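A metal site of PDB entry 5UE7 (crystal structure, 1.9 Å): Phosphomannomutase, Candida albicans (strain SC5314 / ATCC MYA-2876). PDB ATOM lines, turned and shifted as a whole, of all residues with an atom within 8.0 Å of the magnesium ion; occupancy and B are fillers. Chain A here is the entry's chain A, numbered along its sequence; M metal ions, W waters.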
ATOM      1  N   PHE A  15      21.142 -12.645  20.407  1.00  0.00           N
ATOM      2  CA  PHE A  15      20.097 -12.961  19.445  1.00  0.00           C
ATOM      3  C   PHE A  15      20.607 -13.971  18.442  1.00  0.00           C
ATOM      4  O   PHE A  15      21.640 -13.742  17.810  1.00  0.00           O
ATOM      5  CB  PHE A  15      19.632 -11.736  18.678  1.00  0.00           C
ATOM      6  CG  PHE A  15      19.049 -10.670  19.539  1.00  0.00           C
ATOM      7  CD1 PHE A  15      19.865  -9.693  20.074  1.00  0.00           C
ATOM      8  CD2 PHE A  15      17.692 -10.643  19.792  1.00  0.00           C
ATOM      9  CE1 PHE A  15      19.321  -8.701  20.869  1.00  0.00           C
ATOM     10  CE2 PHE A  15      17.148  -9.651  20.588  1.00  0.00           C
ATOM     11  CZ  PHE A  15      17.951  -8.680  21.122  1.00  0.00           C
ATOM     12  N   ASP A  16      19.864 -15.047  18.242  1.00  0.00           N
ATOM     13  CA  ASP A  16      19.976 -15.740  16.973  1.00  0.00           C
ATOM     14  C   ASP A  16      19.651 -14.770  15.856  1.00  0.00           C
ATOM     15  O   ASP A  16      18.873 -13.817  16.032  1.00  0.00           O
ATOM     16  CB  ASP A  16      19.043 -16.949  16.940  1.00  0.00           C
ATOM     17  CG  ASP A  16      18.903 -17.523  15.549  1.00  0.00           C
ATOM     18  OD1 ASP A  16      19.902 -18.033  15.008  1.00  0.00           O
ATOM     19  OD2 ASP A  16      17.780 -17.461  15.010  1.00  0.00           O
ATOM     20  N   VAL A  17      20.269 -14.955  14.694  1.00  0.00           N
ATOM     21  CA  VAL A  17      20.063 -14.007  13.600  1.00  0.00           C
ATOM     22  C   VAL A  17      18.837 -14.407  12.791  1.00  0.00           C
ATOM     23  O   VAL A  17      17.791 -13.752  12.849  1.00  0.00           O
ATOM     24  CB  VAL A  17      21.298 -13.889  12.695  1.00  0.00           C
ATOM     25  CG1 VAL A  17      21.009 -12.926  11.553  1.00  0.00           C
ATOM     26  CG2 VAL A  17      22.504 -13.410  13.487  1.00  0.00           C
ATOM     27  N   ASP A  18      18.962 -15.493  12.017  1.00  0.00           N
ATOM     28  CA  ASP A  18      17.922 -15.872  11.064  1.00  0.00           C
ATOM     29  C   ASP A  18      16.633 -16.248  11.774  1.00  0.00           C
ATOM     30  O   ASP A  18      16.607 -17.168  12.594  1.00  0.00           O
ATOM     31  CB  ASP A  18      18.407 -17.028  10.199  1.00  0.00           C
ATOM     32  CG  ASP A  18      17.397 -17.390   9.134  1.00  0.00           C
ATOM     33  OD1 ASP A  18      17.327 -16.659   8.121  1.00  0.00           O
ATOM     34  OD2 ASP A  18      16.661 -18.382   9.322  1.00  0.00           O
ATOM     35  N   GLY A  19      15.544 -15.563  11.410  1.00  0.00           N
ATOM     36  CA  GLY A  19      14.245 -15.866  11.961  1.00  0.00           C
ATOM     37  C   GLY A  19      13.981 -15.260  13.321  1.00  0.00           C
ATOM     38  O   GLY A  19      12.848 -15.378  13.822  1.00  0.00           O
ATOM     39  N   THR A  20      14.969 -14.628  13.936  1.00  0.00           N
ATOM     40  CA  THR A  20      14.815 -13.965  15.224  1.00  0.00           C
ATOM     41  C   THR A  20      14.985 -12.458  15.099  1.00  0.00           C
ATOM     42  O   THR A  20      14.115 -11.708  15.529  1.00  0.00           O
ATOM     43  CB  THR A  20      15.827 -14.534  16.231  1.00  0.00           C
ATOM     44  OG1 THR A  20      15.638 -15.950  16.359  1.00  0.00           O
ATOM     45  CG2 THR A  20      15.658 -13.883  17.603  1.00  0.00           C
ATOM     46  N   LEU A  21      16.090 -12.004  14.515  1.00  0.00           N
ATOM     47  CA  LEU A  21      16.298 -10.590  14.225  1.00  0.00           C
ATOM     48  C   LEU A  21      15.788 -10.209  12.849  1.00  0.00           C
ATOM     49  O   LEU A  21      15.452  -9.044  12.612  1.00  0.00           O
ATOM     50  CB  LEU A  21      17.778 -10.239  14.317  1.00  0.00           C
ATOM     51  CG  LEU A  21      18.399 -10.125  15.715  1.00  0.00           C
ATOM     52  CD1 LEU A  21      19.876  -9.810  15.610  1.00  0.00           C
ATOM     53  CD2 LEU A  21      17.663  -9.078  16.530  1.00  0.00           C
ATOM     54  N   THR A  22      15.755 -11.157  11.925  1.00  0.00           N
ATOM     55  CA  THR A  22      15.295 -10.984  10.559  1.00  0.00           C
ATOM     56  C   THR A  22      14.138 -11.936  10.296  1.00  0.00           C
ATOM     57  O   THR A  22      13.912 -12.886  11.059  1.00  0.00           O
ATOM     58  CB  THR A  22      16.421 -11.288   9.559  1.00  0.00           C
ATOM     59  OG1 THR A  22      16.489 -12.706   9.337  1.00  0.00           O
ATOM     60  CG2 THR A  22      17.756 -10.799  10.083  1.00  0.00           C
ATOM     61  N   PRO A  23      13.375 -11.720   9.218  1.00  0.00           N
ATOM     62  CA  PRO A  23      12.407 -12.738   8.793  1.00  0.00           C
ATOM     63  C   PRO A  23      13.072 -14.064   8.450  1.00  0.00           C
ATOM     64  O   PRO A  23      14.301 -14.174   8.509  1.00  0.00           O
ATOM     65  CB  PRO A  23      11.755 -12.105   7.555  1.00  0.00           C
ATOM     66  CG  PRO A  23      11.865 -10.635   7.803  1.00  0.00           C
ATOM     67  CD  PRO A  23      13.186 -10.440   8.506  1.00  0.00           C
ATOM     68  N   ALA A  24      12.256 -15.042   8.064  1.00  0.00           N
ATOM     69  CA  ALA A  24      12.724 -16.424   7.928  1.00  0.00           C
ATOM     70  C   ALA A  24      13.973 -16.541   7.059  1.00  0.00           C
ATOM     71  O   ALA A  24      14.842 -17.379   7.327  1.00  0.00           O
ATOM     72  CB  ALA A  24      11.608 -17.289   7.353  1.00  0.00           C
ATOM     73  N   VAL A  48      24.433 -14.248  17.586  1.00  0.00           N
ATOM     74  CA  VAL A  48      25.161 -15.485  17.315  1.00  0.00           C
ATOM     75  C   VAL A  48      24.414 -16.255  16.233  1.00  0.00           C
ATOM     76  O   VAL A  48      23.190 -16.442  16.325  1.00  0.00           O
ATOM     77  CB  VAL A  48      25.369 -16.357  18.563  1.00  0.00           C
ATOM     78  CG1 VAL A  48      24.042 -16.605  19.302  1.00  0.00           C
ATOM     79  CG2 VAL A  48      26.070 -17.656  18.207  1.00  0.00           C
ATOM     80  N   GLY A  49      25.133 -16.673  15.200  1.00  0.00           N
ATOM     81  CA  GLY A  49      24.561 -17.450  14.131  1.00  0.00           C
ATOM     82  C   GLY A  49      25.560 -18.485  13.654  1.00  0.00           C
ATOM     83  O   GLY A  49      26.771 -18.341  13.846  1.00  0.00           O
ATOM     84  N   GLN A  59      22.205 -10.489   5.978  1.00  0.00           N
ATOM     85  CA  GLN A  59      21.037 -10.411   6.854  1.00  0.00           C
ATOM     86  C   GLN A  59      21.023  -9.158   7.723  1.00  0.00           C
ATOM     87  O   GLN A  59      19.963  -8.535   7.888  1.00  0.00           O
ATOM     88  CB  GLN A  59      20.971 -11.654   7.752  1.00  0.00           C
ATOM     89  CG  GLN A  59      20.851 -12.973   7.016  1.00  0.00           C
ATOM     90  CD  GLN A  59      21.201 -14.167   7.901  1.00  0.00           C
ATOM     91  OE1 GLN A  59      22.330 -14.285   8.379  1.00  0.00           O
ATOM     92  NE2 GLN A  59      20.232 -15.046   8.104  1.00  0.00           N
ATOM     93  N   LYS A 193      25.798 -23.244  19.313  1.00  0.00           N
ATOM     94  CA  LYS A 193      25.680 -21.839  19.688  1.00  0.00           C
ATOM     95  C   LYS A 193      26.220 -21.553  21.088  1.00  0.00           C
ATOM     96  O   LYS A 193      26.676 -20.440  21.351  1.00  0.00           O
ATOM     97  CB  LYS A 193      24.213 -21.400  19.594  1.00  0.00           C
ATOM     98  CG  LYS A 193      23.738 -21.038  18.185  1.00  0.00           C
ATOM     99  CD  LYS A 193      22.529 -20.103  18.266  1.00  0.00           C
ATOM    100  CE  LYS A 193      22.093 -19.599  16.899  1.00  0.00           C
ATOM    101  NZ  LYS A 193      21.422 -20.648  16.079  1.00  0.00           N
ATOM    102  N   PHE A 210      18.906 -14.734  25.872  1.00  0.00           N
ATOM    103  CA  PHE A 210      19.029 -15.239  24.513  1.00  0.00           C
ATOM    104  C   PHE A 210      17.652 -15.324  23.874  1.00  0.00           C
ATOM    105  O   PHE A 210      16.705 -15.835  24.493  1.00  0.00           O
ATOM    106  CB  PHE A 210      19.722 -16.611  24.450  1.00  0.00           C
ATOM    107  CG  PHE A 210      19.569 -17.278  23.097  1.00  0.00           C
ATOM    108  CD1 PHE A 210      20.487 -17.005  22.093  1.00  0.00           C
ATOM    109  CD2 PHE A 210      18.612 -18.245  22.870  1.00  0.00           C
ATOM    110  CE1 PHE A 210      20.389 -17.605  20.855  1.00  0.00           C
ATOM    111  CE2 PHE A 210      18.517 -18.867  21.626  1.00  0.00           C
ATOM    112  CZ  PHE A 210      19.400 -18.554  20.633  1.00  0.00           C
ATOM    113  N   PHE A 211      17.560 -14.850  22.640  1.00  0.00           N
ATOM    114  CA  PHE A 211      16.357 -14.899  21.822  1.00  0.00           C
ATOM    115  C   PHE A 211      16.651 -15.789  20.629  1.00  0.00           C
ATOM    116  O   PHE A 211      17.661 -15.606  19.954  1.00  0.00           O
ATOM    117  CB  PHE A 211      15.968 -13.487  21.332  1.00  0.00           C
ATOM    118  CG  PHE A 211      15.334 -12.620  22.386  1.00  0.00           C
ATOM    119  CD1 PHE A 211      16.098 -12.078  23.406  1.00  0.00           C
ATOM    120  CD2 PHE A 211      13.969 -12.340  22.347  1.00  0.00           C
ATOM    121  CE1 PHE A 211      15.516 -11.280  24.381  1.00  0.00           C
ATOM    122  CE2 PHE A 211      13.388 -11.542  23.323  1.00  0.00           C
ATOM    123  CZ  PHE A 211      14.153 -11.020  24.350  1.00  0.00           C
ATOM    124  N   GLY A 212      15.774 -16.755  20.366  1.00  0.00           N
ATOM    125  CA  GLY A 212      15.955 -17.629  19.214  1.00  0.00           C
ATOM    126  C   GLY A 212      14.657 -18.239  18.767  1.00  0.00           C
ATOM    127  O   GLY A 212      13.756 -18.506  19.566  1.00  0.00           O
ATOM    128  N   ASP A 213      14.561 -18.500  17.462  1.00  0.00           N
ATOM    129  CA  ASP A 213      13.332 -18.988  16.868  1.00  0.00           C
ATOM    130  C   ASP A 213      13.283 -20.501  16.711  1.00  0.00           C
ATOM    131  O   ASP A 213      12.251 -21.030  16.288  1.00  0.00           O
ATOM    132  CB  ASP A 213      13.094 -18.337  15.497  1.00  0.00           C
ATOM    133  CG  ASP A 213      14.132 -18.750  14.451  1.00  0.00           C
ATOM    134  OD1 ASP A 213      15.319 -18.860  14.813  1.00  0.00           O
ATOM    135  OD2 ASP A 213      13.748 -18.949  13.280  1.00  0.00           O
ATOM    136  N   LYS A 214      14.349 -21.232  17.046  1.00  0.00           N
ATOM    137  CA  LYS A 214      14.381 -22.684  16.908  1.00  0.00           C
ATOM    138  C   LYS A 214      14.966 -23.313  18.183  1.00  0.00           C
ATOM    139  O   LYS A 214      15.934 -24.058  18.157  1.00  0.00           O
ATOM    140  CB  LYS A 214      15.156 -23.112  15.659  1.00  0.00           C
ATOM    141  CG  LYS A 214      14.671 -22.473  14.341  1.00  0.00           C
ATOM    142  CD  LYS A 214      13.613 -23.309  13.614  1.00  0.00           C
ATOM    143  CE  LYS A 214      13.055 -22.577  12.380  1.00  0.00           C
ATOM    144  NZ  LYS A 214      11.990 -23.350  11.657  1.00  0.00           N
ATOM    145  N   SER A 215      14.326 -22.996  19.318  1.00  0.00           N
ATOM    146  CA  SER A 215      14.714 -23.492  20.639  1.00  0.00           C
ATOM    147  C   SER A 215      14.164 -24.877  20.945  1.00  0.00           C
ATOM    148  O   SER A 215      14.368 -25.373  22.060  1.00  0.00           O
ATOM    149  CB  SER A 215      14.210 -22.540  21.729  1.00  0.00           C
ATOM    150  OG  SER A 215      12.883 -22.146  21.477  1.00  0.00           O
ATOM    151  N   ASN A 220      18.685 -25.378  16.245  1.00  0.00           N
ATOM    152  CA  ASN A 220      20.041 -24.918  16.509  1.00  0.00           C
ATOM    153  C   ASN A 220      20.112 -23.895  17.640  1.00  0.00           C
ATOM    154  O   ASN A 220      21.214 -23.418  17.963  1.00  0.00           O
ATOM    155  CB  ASN A 220      20.677 -24.341  15.234  1.00  0.00           C
ATOM    156  CG  ASN A 220      19.865 -23.212  14.608  1.00  0.00           C
ATOM    157  OD1 ASN A 220      19.093 -22.534  15.275  1.00  0.00           O
ATOM    158  ND2 ASN A 220      20.043 -23.025  13.310  1.00  0.00           N
ATOM    159  N   ASP A 221      18.980 -23.543  18.248  1.00  0.00           N
ATOM    160  CA  ASP A 221      18.948 -22.729  19.455  1.00  0.00           C
ATOM    161  C   ASP A 221      18.734 -23.553  20.719  1.00  0.00           C
ATOM    162  O   ASP A 221      18.771 -22.989  21.819  1.00  0.00           O
ATOM    163  CB  ASP A 221      17.848 -21.667  19.341  1.00  0.00           C
ATOM    164  CG  ASP A 221      18.041 -20.760  18.151  1.00  0.00           C
ATOM    165  OD1 ASP A 221      19.194 -20.410  17.843  1.00  0.00           O
ATOM    166  OD2 ASP A 221      17.030 -20.387  17.511  1.00  0.00           O
ATOM    167  N   VAL A 235      10.950 -17.166  20.303  1.00  0.00           N
ATOM    168  CA  VAL A 235      10.185 -16.274  19.432  1.00  0.00           C
ATOM    169  C   VAL A 235       9.843 -17.014  18.152  1.00  0.00           C
ATOM    170  O   VAL A 235      10.382 -18.075  17.848  1.00  0.00           O
ATOM    171  CB  VAL A 235      10.957 -14.976  19.110  1.00  0.00           C
ATOM    172  CG1 VAL A 235      11.161 -14.137  20.363  1.00  0.00           C
ATOM    173  CG2 VAL A 235      12.286 -15.307  18.446  1.00  0.00           C
HETATM  174 MG    MG M   1      17.060 -18.842  13.686  1.00  0.00          MG
HETATM  175  O   HOH W   1      17.464 -20.312  15.037  1.00  0.00           O
HETATM  176  O   HOH W   2      18.761 -19.116  12.771  1.00  0.00           O
HETATM  177  O   HOH W   3      16.008 -19.615  11.850  1.00  0.00           O
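The side-chain hydroxyl of Thr 20 lies close to the side-chain carboxylate of Asp 16, 2.9 Å away. N of Asp 16 lies within hydrogen-bond range of O of Phe 211 (2.8 Å). The side-chain carboxylate (OD1) of Asp 18 lies close to the backbone carbonyl oxygen (O) of Ala 24, at 2.7 Å. OD1 of Asp 16 lies within salt-bridge range of NZ of Lys 193 (3.2 Å). OD1 of Asp 18 lies within hydrogen-bond range of NE2 of Gln 59 (3.3 Å). N of Asp 213 lies within hydrogen-bond range of OD2 of Asp 221, 3.1 Å away. The backbone NH (N) of Asp 213 is in hydrogen-bond range of the side-chain hydroxyl (OG1) of Thr 20, at 3.0 Å.
Of the 23 residues printed, 3 come within 4 Å of the magnesium ion.
The magnesium ion is bound by water W2 (2.0 Å), water W1 (2.0 Å), the side-chain carboxylate (OD2) of Asp 16 (2.0 Å), the backbone carbonyl oxygen (O) of Asp 18 (2.0 Å), the side-chain carboxylate (OD1) of Asp 213 (2.1 Å) and water W3 (2.3 Å). The magnesium ion has six donor atoms within binding distance.
Water W3 lies within hydrogen-bond range of the side-chain carboxylate (OD2) of Asp 213 (2.8 Å) and the side-chain carboxylate (OD2) of Asp 18 (2.9 Å).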
